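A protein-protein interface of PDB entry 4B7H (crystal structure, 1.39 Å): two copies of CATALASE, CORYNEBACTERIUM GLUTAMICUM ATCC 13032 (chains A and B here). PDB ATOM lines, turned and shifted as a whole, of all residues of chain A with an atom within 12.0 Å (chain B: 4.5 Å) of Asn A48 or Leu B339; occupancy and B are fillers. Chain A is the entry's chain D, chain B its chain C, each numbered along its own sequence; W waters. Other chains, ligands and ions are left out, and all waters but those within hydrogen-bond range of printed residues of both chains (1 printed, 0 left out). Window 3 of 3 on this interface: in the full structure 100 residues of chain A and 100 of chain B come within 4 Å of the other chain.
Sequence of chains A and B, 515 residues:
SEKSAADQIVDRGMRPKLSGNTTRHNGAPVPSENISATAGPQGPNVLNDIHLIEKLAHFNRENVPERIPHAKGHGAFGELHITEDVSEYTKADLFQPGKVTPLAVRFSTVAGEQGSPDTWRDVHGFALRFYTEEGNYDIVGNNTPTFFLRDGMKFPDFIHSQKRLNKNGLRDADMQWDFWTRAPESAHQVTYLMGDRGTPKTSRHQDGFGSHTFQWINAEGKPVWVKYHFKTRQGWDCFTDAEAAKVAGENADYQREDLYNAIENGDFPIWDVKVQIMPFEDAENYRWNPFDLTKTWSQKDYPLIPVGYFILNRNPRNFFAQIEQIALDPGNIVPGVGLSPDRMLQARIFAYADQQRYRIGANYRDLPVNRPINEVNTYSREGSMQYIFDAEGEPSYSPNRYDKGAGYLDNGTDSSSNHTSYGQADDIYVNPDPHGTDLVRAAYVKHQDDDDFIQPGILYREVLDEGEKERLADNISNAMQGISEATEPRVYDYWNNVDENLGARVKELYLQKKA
Hydrophobic or aromatic side chains of chain A that line the printed part of chain B: Ala A28, Ala A37, Leu A47 and Ile A50. Of the 12 printed residues of chain B, 5 touch a printed residue of chain A. Printed residues of chain B that touch a printed residue of chain A: Ile B333, Leu B339, Gln B346, Ile B349 and Ile B428. Among the printed residues, 11 pairs touch across the chains. Among the printed residues, no Asp or Glu carboxylate lies within 4 Å of a Lys or Arg side-chain nitrogen of the other chain.
Printed residues of chain B within 4 Å of Ala A28: Ile B333 (3.6 Å). Of the printed residues of chain B, Ala A37 touches Ile B428. Of the printed residues of chain B, Leu A47 touches Gln B346 (3.6 Å). Printed residues of chain B within 4 Å of Ile A50: Ile B333 (3.98 Å) and Ile B349 (3.6 Å). No residue of chain A comes within 4 Å of Phe B214. No residue of chain A comes within 4 Å of Gln B215. No residue of chain A comes within 4 Å of Gly B338. Of chain A, only Asn A48 comes within 4 Å of Leu B339. No residue of chain A comes within 4 Å of Ser B340. No residue of chain A comes within 4 Å of Leu B345. Of the printed residues of chain A, Gln B346 touches Leu A47 and Asn A48. Ile B428 touches just these residues of chain A: Ala A37 and Asn A48. No residue of chain A comes within 4 Å of Tyr B429. The nearest printed residue of chain B that does not touch Asn A48 is Leu B345 (5.1 Å). The nearest residue of chain A that does not touch Leu B339 is Ile A50 (4.9 Å).
No position is printed for both chains. Of the 11 pairs that touch across the chains among the printed residues, none has its exchanged pair printed and touching as well.
The backbone carbonyl oxygen (O) of Gln B346 lies close to the side-chain amide oxygen (OD1) of Asn A48, 2.9 Å away. O of Ile B333 sits at hydrogen-bond distance from ND2 of Asn A26 (3.1 Å). The backbone carbonyl oxygen (O) of Ile B333 sits at hydrogen-bond distance from the guanidinium group (NH2) of Arg A24 (3.4 Å).
The side-chain amide oxygen of Asn A26 lies within hydrogen-bond range of the backbone NH of Ala A28, 3.0 Å away. O of Ser B340 lies within hydrogen-bond range of NE2 of Gln B346 (2.9 Å). O of Ile B428 is in hydrogen-bond range of N of Leu B339. The backbone NH of Val A46 is in hydrogen-bond range of the backbone carbonyl oxygen of Ala A37 (3.2 Å).
CB of Ala A28 touches O of Ile B333 (3.6 Å). Ile B428 touches Ala A37 (CD1 to CB, 3.7 Å). Gln B346 touches Leu A47. Leu B339 touches Asn A48 (CD1 to ND2, 3.7 Å). Ile B349 touches Asn A48. O of Asn A48 touches CD1 of Ile B428 (3.6 Å). Ile A50 touches Ile B333 (CD1 to CD1, 3.98 Å). CG1 of Ile A50 touches CG2 of Ile B349, 3.6 Å away.
Water W1 lies within hydrogen-bond range of the side-chain amide oxygen (OE1) of Gln B346 (2.9 Å), the backbone NH (N) of Asn A48 (2.9 Å) and the backbone NH (N) of Leu A47 (3.2 Å).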
ATOM      1  N   ARG A  24      16.095  13.263 -19.436  1.00  0.00           N
ATOM      2  CA  ARG A  24      15.748  13.831 -20.734  1.00  0.00           C
ATOM      3  C   ARG A  24      14.399  14.535 -20.611  1.00  0.00           C
ATOM      4  O   ARG A  24      13.753  14.494 -19.555  1.00  0.00           O
ATOM      5  CB  ARG A  24      15.709  12.754 -21.823  1.00  0.00           C
ATOM      6  CG  ARG A  24      17.044  12.055 -22.004  1.00  0.00           C
ATOM      7  CD  ARG A  24      17.203  11.464 -23.397  1.00  0.00           C
ATOM      8  NE  ARG A  24      15.966  10.881 -23.896  1.00  0.00           N
ATOM      9  CZ  ARG A  24      15.572   9.633 -23.676  1.00  0.00           C
ATOM     10  NH1 ARG A  24      16.314   8.806 -22.949  1.00  0.00           N
ATOM     11  NH2 ARG A  24      14.425   9.207 -24.190  1.00  0.00           N
ATOM     12  N   ASN A  26      11.613  13.802 -21.843  1.00  0.00           N
ATOM     13  CA  ASN A  26      10.510  12.870 -21.613  1.00  0.00           C
ATOM     14  C   ASN A  26      10.490  12.323 -20.183  1.00  0.00           C
ATOM     15  O   ASN A  26       9.585  11.560 -19.834  1.00  0.00           O
ATOM     16  CB  ASN A  26      10.544  11.698 -22.599  1.00  0.00           C
ATOM     17  CG  ASN A  26      11.607  10.669 -22.253  1.00  0.00           C
ATOM     18  OD1 ASN A  26      12.684  11.018 -21.771  1.00  0.00           O
ATOM     19  ND2 ASN A  26      11.312   9.393 -22.508  1.00  0.00           N
ATOM     20  N   ALA A  28      12.961  10.399 -18.802  1.00  0.00           N
ATOM     21  CA  ALA A  28      13.828   9.224 -18.652  1.00  0.00           C
ATOM     22  C   ALA A  28      15.221   9.636 -18.165  1.00  0.00           C
ATOM     23  O   ALA A  28      15.696  10.719 -18.498  1.00  0.00           O
ATOM     24  CB  ALA A  28      13.917   8.448 -19.961  1.00  0.00           C
ATOM     25  N   PRO A  29      15.883   8.778 -17.367  1.00  0.00           N
ATOM     26  CA  PRO A  29      17.206   9.122 -16.821  1.00  0.00           C
ATOM     27  C   PRO A  29      18.275   9.370 -17.896  1.00  0.00           C
ATOM     28  O   PRO A  29      18.353   8.636 -18.890  1.00  0.00           O
ATOM     29  CB  PRO A  29      17.575   7.889 -15.983  1.00  0.00           C
ATOM     30  CG  PRO A  29      16.251   7.271 -15.624  1.00  0.00           C
ATOM     31  CD  PRO A  29      15.367   7.511 -16.819  1.00  0.00           C
ATOM     32  N   VAL A  30      19.085  10.410 -17.690  1.00  0.00           N
ATOM     33  CA  VAL A  30      20.216  10.703 -18.570  1.00  0.00           C
ATOM     34  C   VAL A  30      21.413   9.850 -18.181  1.00  0.00           C
ATOM     35  O   VAL A  30      21.815   9.865 -17.022  1.00  0.00           O
ATOM     36  CB  VAL A  30      20.634  12.195 -18.461  1.00  0.00           C
ATOM     37  CG1 VAL A  30      22.004  12.428 -19.089  1.00  0.00           C
ATOM     38  CG2 VAL A  30      19.595  13.108 -19.094  1.00  0.00           C
ATOM     39  N   PRO A  31      21.994   9.105 -19.142  1.00  0.00           N
ATOM     40  CA  PRO A  31      23.201   8.338 -18.806  1.00  0.00           C
ATOM     41  C   PRO A  31      24.410   9.238 -18.520  1.00  0.00           C
ATOM     42  O   PRO A  31      25.062   9.072 -17.482  1.00  0.00           O
ATOM     43  CB  PRO A  31      23.434   7.473 -20.055  1.00  0.00           C
ATOM     44  CG  PRO A  31      22.075   7.387 -20.710  1.00  0.00           C
ATOM     45  CD  PRO A  31      21.464   8.741 -20.466  1.00  0.00           C
ATOM     46  N   SER A  32      24.703  10.190 -19.401  1.00  0.00           N
ATOM     47  CA  SER A  32      25.861  11.050 -19.181  1.00  0.00           C
ATOM     48  C   SER A  32      25.667  12.464 -19.698  1.00  0.00           C
ATOM     49  O   SER A  32      25.088  12.670 -20.767  1.00  0.00           O
ATOM     50  CB  SER A  32      27.105  10.449 -19.850  1.00  0.00           C
ATOM     51  OG  SER A  32      28.263  11.223 -19.561  1.00  0.00           O
ATOM     52  N   ILE A  35      29.966  12.449 -21.838  1.00  0.00           N
ATOM     53  CA  ILE A  35      30.524  11.657 -22.929  1.00  0.00           C
ATOM     54  C   ILE A  35      29.408  11.237 -23.886  1.00  0.00           C
ATOM     55  O   ILE A  35      28.354  10.769 -23.445  1.00  0.00           O
ATOM     56  CB  ILE A  35      31.229  10.397 -22.387  1.00  0.00           C
ATOM     57  CG1 ILE A  35      32.310  10.783 -21.371  1.00  0.00           C
ATOM     58  CG2 ILE A  35      31.819   9.575 -23.517  1.00  0.00           C
ATOM     59  CD1 ILE A  35      33.038   9.593 -20.770  1.00  0.00           C
ATOM     60  N   SER A  36      29.622  11.445 -25.183  1.00  0.00           N
ATOM     61  CA  SER A  36      28.648  11.031 -26.193  1.00  0.00           C
ATOM     62  C   SER A  36      28.935   9.617 -26.702  1.00  0.00           C
ATOM     63  O   SER A  36      30.056   9.113 -26.555  1.00  0.00           O
ATOM     64  CB  SER A  36      28.578  12.039 -27.354  1.00  0.00           C
ATOM     65  OG  SER A  36      29.843  12.274 -27.955  1.00  0.00           O
ATOM     66  N   ALA A  37      27.918   8.972 -27.272  1.00  0.00           N
ATOM     67  CA  ALA A  37      28.028   7.575 -27.684  1.00  0.00           C
ATOM     68  C   ALA A  37      28.634   7.421 -29.072  1.00  0.00           C
ATOM     69  O   ALA A  37      28.244   8.100 -30.019  1.00  0.00           O
ATOM     70  CB  ALA A  37      26.679   6.900 -27.622  1.00  0.00           C
ATOM     71  N   THR A  38      29.569   6.492 -29.199  1.00  0.00           N
ATOM     72  CA  THR A  38      30.253   6.271 -30.461  1.00  0.00           C
ATOM     73  C   THR A  38      30.268   4.779 -30.794  1.00  0.00           C
ATOM     74  O   THR A  38      30.124   3.929 -29.909  1.00  0.00           O
ATOM     75  CB  THR A  38      31.706   6.805 -30.397  1.00  0.00           C
ATOM     76  OG1 THR A  38      32.382   6.214 -29.279  1.00  0.00           O
ATOM     77  CG2 THR A  38      31.729   8.322 -30.238  1.00  0.00           C
ATOM     78  N   ALA A  39      30.452   4.462 -32.072  1.00  0.00           N
ATOM     79  CA  ALA A  39      30.566   3.071 -32.501  1.00  0.00           C
ATOM     80  C   ALA A  39      32.028   2.634 -32.385  1.00  0.00           C
ATOM     81  O   ALA A  39      32.785   2.685 -33.361  1.00  0.00           O
ATOM     82  CB  ALA A  39      30.052   2.916 -33.917  1.00  0.00           C
ATOM     83  N   GLY A  43      35.461   5.242 -33.028  1.00  0.00           N
ATOM     84  CA  GLY A  43      34.492   5.199 -34.106  1.00  0.00           C
ATOM     85  C   GLY A  43      33.661   6.466 -34.209  1.00  0.00           C
ATOM     86  O   GLY A  43      33.783   7.382 -33.392  1.00  0.00           O
ATOM     87  N   PRO A  44      32.799   6.525 -35.228  1.00  0.00           N
ATOM     88  CA  PRO A  44      31.963   7.714 -35.437  1.00  0.00           C
ATOM     89  C   PRO A  44      30.909   7.885 -34.345  1.00  0.00           C
ATOM     90  O   PRO A  44      30.464   6.903 -33.739  1.00  0.00           O
ATOM     91  CB  PRO A  44      31.282   7.425 -36.780  1.00  0.00           C
ATOM     92  CG  PRO A  44      31.285   5.919 -36.876  1.00  0.00           C
ATOM     93  CD  PRO A  44      32.562   5.476 -36.234  1.00  0.00           C
ATOM     94  N   ASN A  45      30.521   9.128 -34.085  1.00  0.00           N
ATOM     95  CA  ASN A  45      29.363   9.390 -33.253  1.00  0.00           C
ATOM     96  C   ASN A  45      28.121   8.782 -33.884  1.00  0.00           C
ATOM     97  O   ASN A  45      27.908   8.908 -35.095  1.00  0.00           O
ATOM     98  CB  ASN A  45      29.174  10.890 -33.054  1.00  0.00           C
ATOM     99  CG  ASN A  45      29.980  11.414 -31.893  1.00  0.00           C
ATOM    100  OD1 ASN A  45      29.452  11.618 -30.797  1.00  0.00           O
ATOM    101  ND2 ASN A  45      31.270  11.592 -32.109  1.00  0.00           N
ATOM    102  N   VAL A  46      27.313   8.114 -33.068  1.00  0.00           N
ATOM    103  CA  VAL A  46      26.086   7.508 -33.565  1.00  0.00           C
ATOM    104  C   VAL A  46      24.979   8.548 -33.629  1.00  0.00           C
ATOM    105  O   VAL A  46      24.962   9.518 -32.863  1.00  0.00           O
ATOM    106  CB  VAL A  46      25.643   6.292 -32.717  1.00  0.00           C
ATOM    107  CG1 VAL A  46      26.767   5.273 -32.653  1.00  0.00           C
ATOM    108  CG2 VAL A  46      25.213   6.719 -31.301  1.00  0.00           C
ATOM    109  N   LEU A  47      24.053   8.348 -34.554  1.00  0.00           N
ATOM    110  CA  LEU A  47      22.918   9.253 -34.684  1.00  0.00           C
ATOM    111  C   LEU A  47      22.051   9.220 -33.424  1.00  0.00           C
ATOM    112  O   LEU A  47      21.593  10.258 -32.948  1.00  0.00           O
ATOM    113  CB  LEU A  47      22.095   8.852 -35.905  1.00  0.00           C
ATOM    114  CG  LEU A  47      20.822   9.653 -36.186  1.00  0.00           C
ATOM    115  CD1 LEU A  47      21.120  11.136 -36.363  1.00  0.00           C
ATOM    116  CD2 LEU A  47      20.115   9.087 -37.414  1.00  0.00           C
ATOM    117  N   ASN A  48      21.867   8.031 -32.857  1.00  0.00           N
ATOM    118  CA  ASN A  48      20.887   7.848 -31.796  1.00  0.00           C
ATOM    119  C   ASN A  48      21.431   8.006 -30.379  1.00  0.00           C
ATOM    120  O   ASN A  48      21.060   7.260 -29.475  1.00  0.00           O
ATOM    121  CB  ASN A  48      20.165   6.511 -31.939  1.00  0.00           C
ATOM    122  CG  ASN A  48      19.423   6.385 -33.253  1.00  0.00           C
ATOM    123  OD1 ASN A  48      19.044   7.385 -33.894  1.00  0.00           O
ATOM    124  ND2 ASN A  48      19.216   5.157 -33.669  1.00  0.00           N
ATOM    125  N   ASP A  49      22.292   8.995 -30.181  1.00  0.00           N
ATOM    126  CA  ASP A  49      22.530   9.472 -28.833  1.00  0.00           C
ATOM    127  C   ASP A  49      21.422  10.492 -28.598  1.00  0.00           C
ATOM    128  O   ASP A  49      21.552  11.668 -28.955  1.00  0.00           O
ATOM    129  CB  ASP A  49      23.928  10.069 -28.678  1.00  0.00           C
ATOM    130  CG  ASP A  49      24.250  10.403 -27.235  1.00  0.00           C
ATOM    131  OD1 ASP A  49      23.310  10.764 -26.489  1.00  0.00           O
ATOM    132  OD2 ASP A  49      25.427  10.283 -26.829  1.00  0.00           O
ATOM    133  N   ILE A  50      20.308  10.017 -28.048  1.00  0.00           N
ATOM    134  CA  ILE A  50      19.090  10.819 -27.963  1.00  0.00           C
ATOM    135  C   ILE A  50      19.316  12.064 -27.114  1.00  0.00           C
ATOM    136  O   ILE A  50      18.945  13.176 -27.502  1.00  0.00           O
ATOM    137  CB  ILE A  50      17.889   9.992 -27.432  1.00  0.00           C
ATOM    138  CG1 ILE A  50      17.666   8.765 -28.325  1.00  0.00           C
ATOM    139  CG2 ILE A  50      16.631  10.853 -27.378  1.00  0.00           C
ATOM    140  CD1 ILE A  50      16.675   7.768 -27.783  1.00  0.00           C
ATOM    141  N   HIS A  51      19.966  11.892 -25.971  1.00  0.00           N
ATOM    142  CA  HIS A  51      20.253  13.029 -25.118  1.00  0.00           C
ATOM    143  C   HIS A  51      21.186  14.048 -25.783  1.00  0.00           C
ATOM    144  O   HIS A  51      20.954  15.258 -25.680  1.00  0.00           O
ATOM    145  CB  HIS A  51      20.825  12.577 -23.780  1.00  0.00           C
ATOM    146  CG  HIS A  51      21.137  13.711 -22.857  1.00  0.00           C
ATOM    147  ND1 HIS A  51      20.188  14.634 -22.465  1.00  0.00           N
ATOM    148  CD2 HIS A  51      22.294  14.081 -22.263  1.00  0.00           C
ATOM    149  CE1 HIS A  51      20.751  15.521 -21.662  1.00  0.00           C
ATOM    150  NE2 HIS A  51      22.028  15.206 -21.521  1.00  0.00           N
ATOM    151  N   LEU A  52      22.235  13.579 -26.458  1.00  0.00           N
ATOM    152  CA  LEU A  52      23.131  14.503 -27.160  1.00  0.00           C
ATOM    153  C   LEU A  52      22.354  15.422 -28.097  1.00  0.00           C
ATOM    154  O   LEU A  52      22.501  16.650 -28.066  1.00  0.00           O
ATOM    155  CB  LEU A  52      24.178  13.748 -27.979  1.00  0.00           C
ATOM    156  CG  LEU A  52      25.111  14.653 -28.798  1.00  0.00           C
ATOM    157  CD1 LEU A  52      26.001  15.510 -27.891  1.00  0.00           C
ATOM    158  CD2 LEU A  52      25.932  13.842 -29.795  1.00  0.00           C
ATOM    159  N   ILE A  53      21.514  14.822 -28.934  1.00  0.00           N
ATOM    160  CA  ILE A  53      20.804  15.609 -29.934  1.00  0.00           C
ATOM    161  C   ILE A  53      19.787  16.545 -29.277  1.00  0.00           C
ATOM    162  O   ILE A  53      19.627  17.697 -29.685  1.00  0.00           O
ATOM    163  CB  ILE A  53      20.149  14.703 -30.995  1.00  0.00           C
ATOM    164  CG1 ILE A  53      21.220  13.846 -31.678  1.00  0.00           C
ATOM    165  CG2 ILE A  53      19.354  15.523 -32.014  1.00  0.00           C
ATOM    166  CD1 ILE A  53      22.362  14.631 -32.279  1.00  0.00           C
ATOM    167  N   GLU A  54      19.111  16.061 -28.241  1.00  0.00           N
ATOM    168  CA  GLU A  54      18.120  16.876 -27.541  1.00  0.00           C
ATOM    169  C   GLU A  54      18.783  18.093 -26.879  1.00  0.00           C
ATOM    170  O   GLU A  54      18.269  19.220 -26.941  1.00  0.00           O
ATOM    171  CB  GLU A  54      17.385  16.018 -26.504  1.00  0.00           C
ATOM    172  CG  GLU A  54      16.241  16.711 -25.786  1.00  0.00           C
ATOM    173  CD  GLU A  54      15.394  15.722 -25.011  1.00  0.00           C
ATOM    174  OE1 GLU A  54      14.506  15.080 -25.612  1.00  0.00           O
ATOM    175  OE2 GLU A  54      15.625  15.559 -23.798  1.00  0.00           O
ATOM    176  N   LYS A  55      19.931  17.852 -26.252  1.00  0.00           N
ATOM    177  CA  LYS A  55      20.708  18.883 -25.563  1.00  0.00           C
ATOM    178  C   LYS A  55      21.222  19.923 -26.557  1.00  0.00           C
ATOM    179  O   LYS A  55      21.084  21.131 -26.335  1.00  0.00           O
ATOM    180  CB  LYS A  55      21.872  18.206 -24.832  1.00  0.00           C
ATOM    181  CG  LYS A  55      22.681  19.118 -23.917  1.00  0.00           C
ATOM    182  CD  LYS A  55      23.674  18.291 -23.096  1.00  0.00           C
ATOM    183  CE  LYS A  55      24.453  19.142 -22.099  1.00  0.00           C
ATOM    184  NZ  LYS A  55      25.324  18.304 -21.231  1.00  0.00           N
ATOM    185  N   LEU A  56      21.783  19.458 -27.670  1.00  0.00           N
ATOM    186  CA  LEU A  56      22.268  20.382 -28.691  1.00  0.00           C
ATOM    187  C   LEU A  56      21.130  21.133 -29.372  1.00  0.00           C
ATOM    188  O   LEU A  56      21.236  22.343 -29.607  1.00  0.00           O
ATOM    189  CB  LEU A  56      23.095  19.655 -29.749  1.00  0.00           C
ATOM    190  CG  LEU A  56      24.426  19.058 -29.294  1.00  0.00           C
ATOM    191  CD1 LEU A  56      25.026  18.264 -30.440  1.00  0.00           C
ATOM    192  CD2 LEU A  56      25.381  20.139 -28.791  1.00  0.00           C
ATOM    193  N   PHE B 214      12.348  -3.970 -31.573  1.00  0.00           N
ATOM    194  CA  PHE B 214      12.911  -3.209 -30.469  1.00  0.00           C
ATOM    195  C   PHE B 214      13.673  -4.171 -29.577  1.00  0.00           C
ATOM    196  O   PHE B 214      13.748  -5.375 -29.861  1.00  0.00           O
ATOM    197  CB  PHE B 214      11.805  -2.498 -29.683  1.00  0.00           C
ATOM    198  CG  PHE B 214      11.121  -1.417 -30.468  1.00  0.00           C
ATOM    199  CD1 PHE B 214      11.681  -0.151 -30.555  1.00  0.00           C
ATOM    200  CD2 PHE B 214       9.931  -1.673 -31.139  1.00  0.00           C
ATOM    201  CE1 PHE B 214      11.070   0.847 -31.298  1.00  0.00           C
ATOM    202  CE2 PHE B 214       9.307  -0.669 -31.877  1.00  0.00           C
ATOM    203  CZ  PHE B 214       9.882   0.585 -31.954  1.00  0.00           C
ATOM    204  N   GLN B 215      14.253  -3.650 -28.507  1.00  0.00           N
ATOM    205  CA  GLN B 215      14.925  -4.506 -27.547  1.00  0.00           C
ATOM    206  C   GLN B 215      14.307  -4.347 -26.170  1.00  0.00           C
ATOM    207  O   GLN B 215      13.898  -3.249 -25.784  1.00  0.00           O
ATOM    208  CB  GLN B 215      16.420  -4.184 -27.509  1.00  0.00           C
ATOM    209  CG  GLN B 215      17.255  -5.245 -26.839  1.00  0.00           C
ATOM    210  CD  GLN B 215      18.727  -4.938 -26.947  1.00  0.00           C
ATOM    211  OE1 GLN B 215      19.259  -4.132 -26.181  1.00  0.00           O
ATOM    212  NE2 GLN B 215      19.403  -5.573 -27.912  1.00  0.00           N
ATOM    213  N   TRP B 225      15.206  -9.505 -28.324  1.00  0.00           N
ATOM    214  CA  TRP B 225      14.558  -8.700 -29.347  1.00  0.00           C
ATOM    215  C   TRP B 225      13.047  -8.890 -29.271  1.00  0.00           C
ATOM    216  O   TRP B 225      12.566 -10.005 -29.051  1.00  0.00           O
ATOM    217  CB  TRP B 225      15.061  -9.100 -30.727  1.00  0.00           C
ATOM    218  CG  TRP B 225      16.540  -8.943 -30.911  1.00  0.00           C
ATOM    219  CD1 TRP B 225      17.445  -9.944 -31.101  1.00  0.00           C
ATOM    220  CD2 TRP B 225      17.285  -7.715 -30.937  1.00  0.00           C
ATOM    221  NE1 TRP B 225      18.706  -9.422 -31.244  1.00  0.00           N
ATOM    222  CE2 TRP B 225      18.636  -8.053 -31.150  1.00  0.00           C
ATOM    223  CE3 TRP B 225      16.939  -6.363 -30.810  1.00  0.00           C
ATOM    224  CZ2 TRP B 225      19.647  -7.094 -31.229  1.00  0.00           C
ATOM    225  CZ3 TRP B 225      17.949  -5.404 -30.890  1.00  0.00           C
ATOM    226  CH2 TRP B 225      19.286  -5.776 -31.101  1.00  0.00           C
ATOM    227  N   ILE B 333      11.927   6.667 -25.331  1.00  0.00           N
ATOM    228  CA  ILE B 333      12.103   5.358 -24.719  1.00  0.00           C
ATOM    229  C   ILE B 333      12.443   5.522 -23.239  1.00  0.00           C
ATOM    230  O   ILE B 333      12.724   6.632 -22.775  1.00  0.00           O
ATOM    231  CB  ILE B 333      13.154   4.495 -25.465  1.00  0.00           C
ATOM    232  CG1 ILE B 333      14.521   5.186 -25.490  1.00  0.00           C
ATOM    233  CG2 ILE B 333      12.674   4.192 -26.881  1.00  0.00           C
ATOM    234  CD1 ILE B 333      15.621   4.319 -26.091  1.00  0.00           C
ATOM    235  N   GLY B 338      15.015  -0.730 -25.601  1.00  0.00           N
ATOM    236  CA  GLY B 338      16.092  -0.270 -26.456  1.00  0.00           C
ATOM    237  C   GLY B 338      15.697  -0.311 -27.921  1.00  0.00           C
ATOM    238  O   GLY B 338      14.605  -0.768 -28.269  1.00  0.00           O
ATOM    239  N   LEU B 339      16.606   0.147 -28.775  1.00  0.00           N
ATOM    240  CA  LEU B 339      16.377   0.186 -30.212  1.00  0.00           C
ATOM    241  C   LEU B 339      16.938  -1.084 -30.861  1.00  0.00           C
ATOM    242  O   LEU B 339      17.055  -2.115 -30.200  1.00  0.00           O
ATOM    243  CB  LEU B 339      17.026   1.442 -30.794  1.00  0.00           C
ATOM    244  CG  LEU B 339      16.674   2.743 -30.069  1.00  0.00           C
ATOM    245  CD1 LEU B 339      17.404   3.914 -30.701  1.00  0.00           C
ATOM    246  CD2 LEU B 339      15.166   2.971 -30.072  1.00  0.00           C
ATOM    247  N   SER B 340      17.285  -1.002 -32.144  1.00  0.00           N
ATOM    248  CA  SER B 340      17.827  -2.128 -32.905  1.00  0.00           C
ATOM    249  C   SER B 340      18.491  -1.555 -34.156  1.00  0.00           C
ATOM    250  O   SER B 340      18.313  -0.365 -34.435  1.00  0.00           O
ATOM    251  CB  SER B 340      16.699  -3.098 -33.283  1.00  0.00           C
ATOM    252  OG  SER B 340      15.941  -2.606 -34.377  1.00  0.00           O
ATOM    253  N   LEU B 345      14.023   2.758 -38.129  1.00  0.00           N
ATOM    254  CA  LEU B 345      13.863   3.138 -36.736  1.00  0.00           C
ATOM    255  C   LEU B 345      14.896   4.193 -36.337  1.00  0.00           C
ATOM    256  O   LEU B 345      14.565   5.193 -35.703  1.00  0.00           O
ATOM    257  CB  LEU B 345      13.982   1.913 -35.837  1.00  0.00           C
ATOM    258  CG  LEU B 345      13.940   2.214 -34.342  1.00  0.00           C
ATOM    259  CD1 LEU B 345      12.657   2.970 -33.981  1.00  0.00           C
ATOM    260  CD2 LEU B 345      14.069   0.904 -33.563  1.00  0.00           C
ATOM    261  N   GLN B 346      16.147   3.985 -36.731  1.00  0.00           N
ATOM    262  CA  GLN B 346      17.208   4.896 -36.319  1.00  0.00           C
ATOM    263  C   GLN B 346      17.019   6.304 -36.897  1.00  0.00           C
ATOM    264  O   GLN B 346      17.257   7.284 -36.210  1.00  0.00           O
ATOM    265  CB  GLN B 346      18.586   4.290 -36.607  1.00  0.00           C
ATOM    266  CG  GLN B 346      18.789   2.985 -35.818  1.00  0.00           C
ATOM    267  CD  GLN B 346      20.239   2.686 -35.457  1.00  0.00           C
ATOM    268  OE1 GLN B 346      21.149   3.475 -35.728  1.00  0.00           O
ATOM    269  NE2 GLN B 346      20.460   1.523 -34.845  1.00  0.00           N
ATOM    270  N   ILE B 349      14.251   8.040 -34.844  1.00  0.00           N
ATOM    271  CA  ILE B 349      14.686   8.515 -33.529  1.00  0.00           C
ATOM    272  C   ILE B 349      15.169   9.974 -33.601  1.00  0.00           C
ATOM    273  O   ILE B 349      15.017  10.734 -32.642  1.00  0.00           O
ATOM    274  CB  ILE B 349      15.753   7.569 -32.901  1.00  0.00           C
ATOM    275  CG1 ILE B 349      15.169   6.169 -32.684  1.00  0.00           C
ATOM    276  CG2 ILE B 349      16.302   8.135 -31.601  1.00  0.00           C
ATOM    277  CD1 ILE B 349      14.000   6.109 -31.727  1.00  0.00           C
ATOM    278  N   ILE B 428      20.829   2.504 -25.209  1.00  0.00           N
ATOM    279  CA  ILE B 428      20.486   2.722 -26.615  1.00  0.00           C
ATOM    280  C   ILE B 428      20.039   1.364 -27.166  1.00  0.00           C
ATOM    281  O   ILE B 428      18.870   1.190 -27.508  1.00  0.00           O
ATOM    282  CB  ILE B 428      21.654   3.346 -27.410  1.00  0.00           C
ATOM    283  CG1 ILE B 428      22.110   4.646 -26.736  1.00  0.00           C
ATOM    284  CG2 ILE B 428      21.242   3.609 -28.860  1.00  0.00           C
ATOM    285  CD1 ILE B 428      23.291   5.322 -27.424  1.00  0.00           C
ATOM    286  N   TYR B 429      20.966   0.407 -27.223  1.00  0.00           N
ATOM    287  CA  TYR B 429      20.624  -1.017 -27.290  1.00  0.00           C
ATOM    288  C   TYR B 429      21.902  -1.810 -27.135  1.00  0.00           C
ATOM    289  O   TYR B 429      22.990  -1.299 -27.413  1.00  0.00           O
ATOM    290  CB  TYR B 429      19.903  -1.423 -28.593  1.00  0.00           C
ATOM    291  CG  TYR B 429      20.635  -1.109 -29.888  1.00  0.00           C
ATOM    292  CD1 TYR B 429      20.644   0.182 -30.402  1.00  0.00           C
ATOM    293  CD2 TYR B 429      21.275  -2.112 -30.619  1.00  0.00           C
ATOM    294  CE1 TYR B 429      21.296   0.480 -31.593  1.00  0.00           C
ATOM    295  CE2 TYR B 429      21.929  -1.824 -31.811  1.00  0.00           C
ATOM    296  CZ  TYR B 429      21.938  -0.524 -32.294  1.00  0.00           C
ATOM    297  OH  TYR B 429      22.586  -0.224 -33.484  1.00  0.00           O
HETATM  298  O   HOH W   1      22.490   5.574 -34.328  1.00  0.00           O
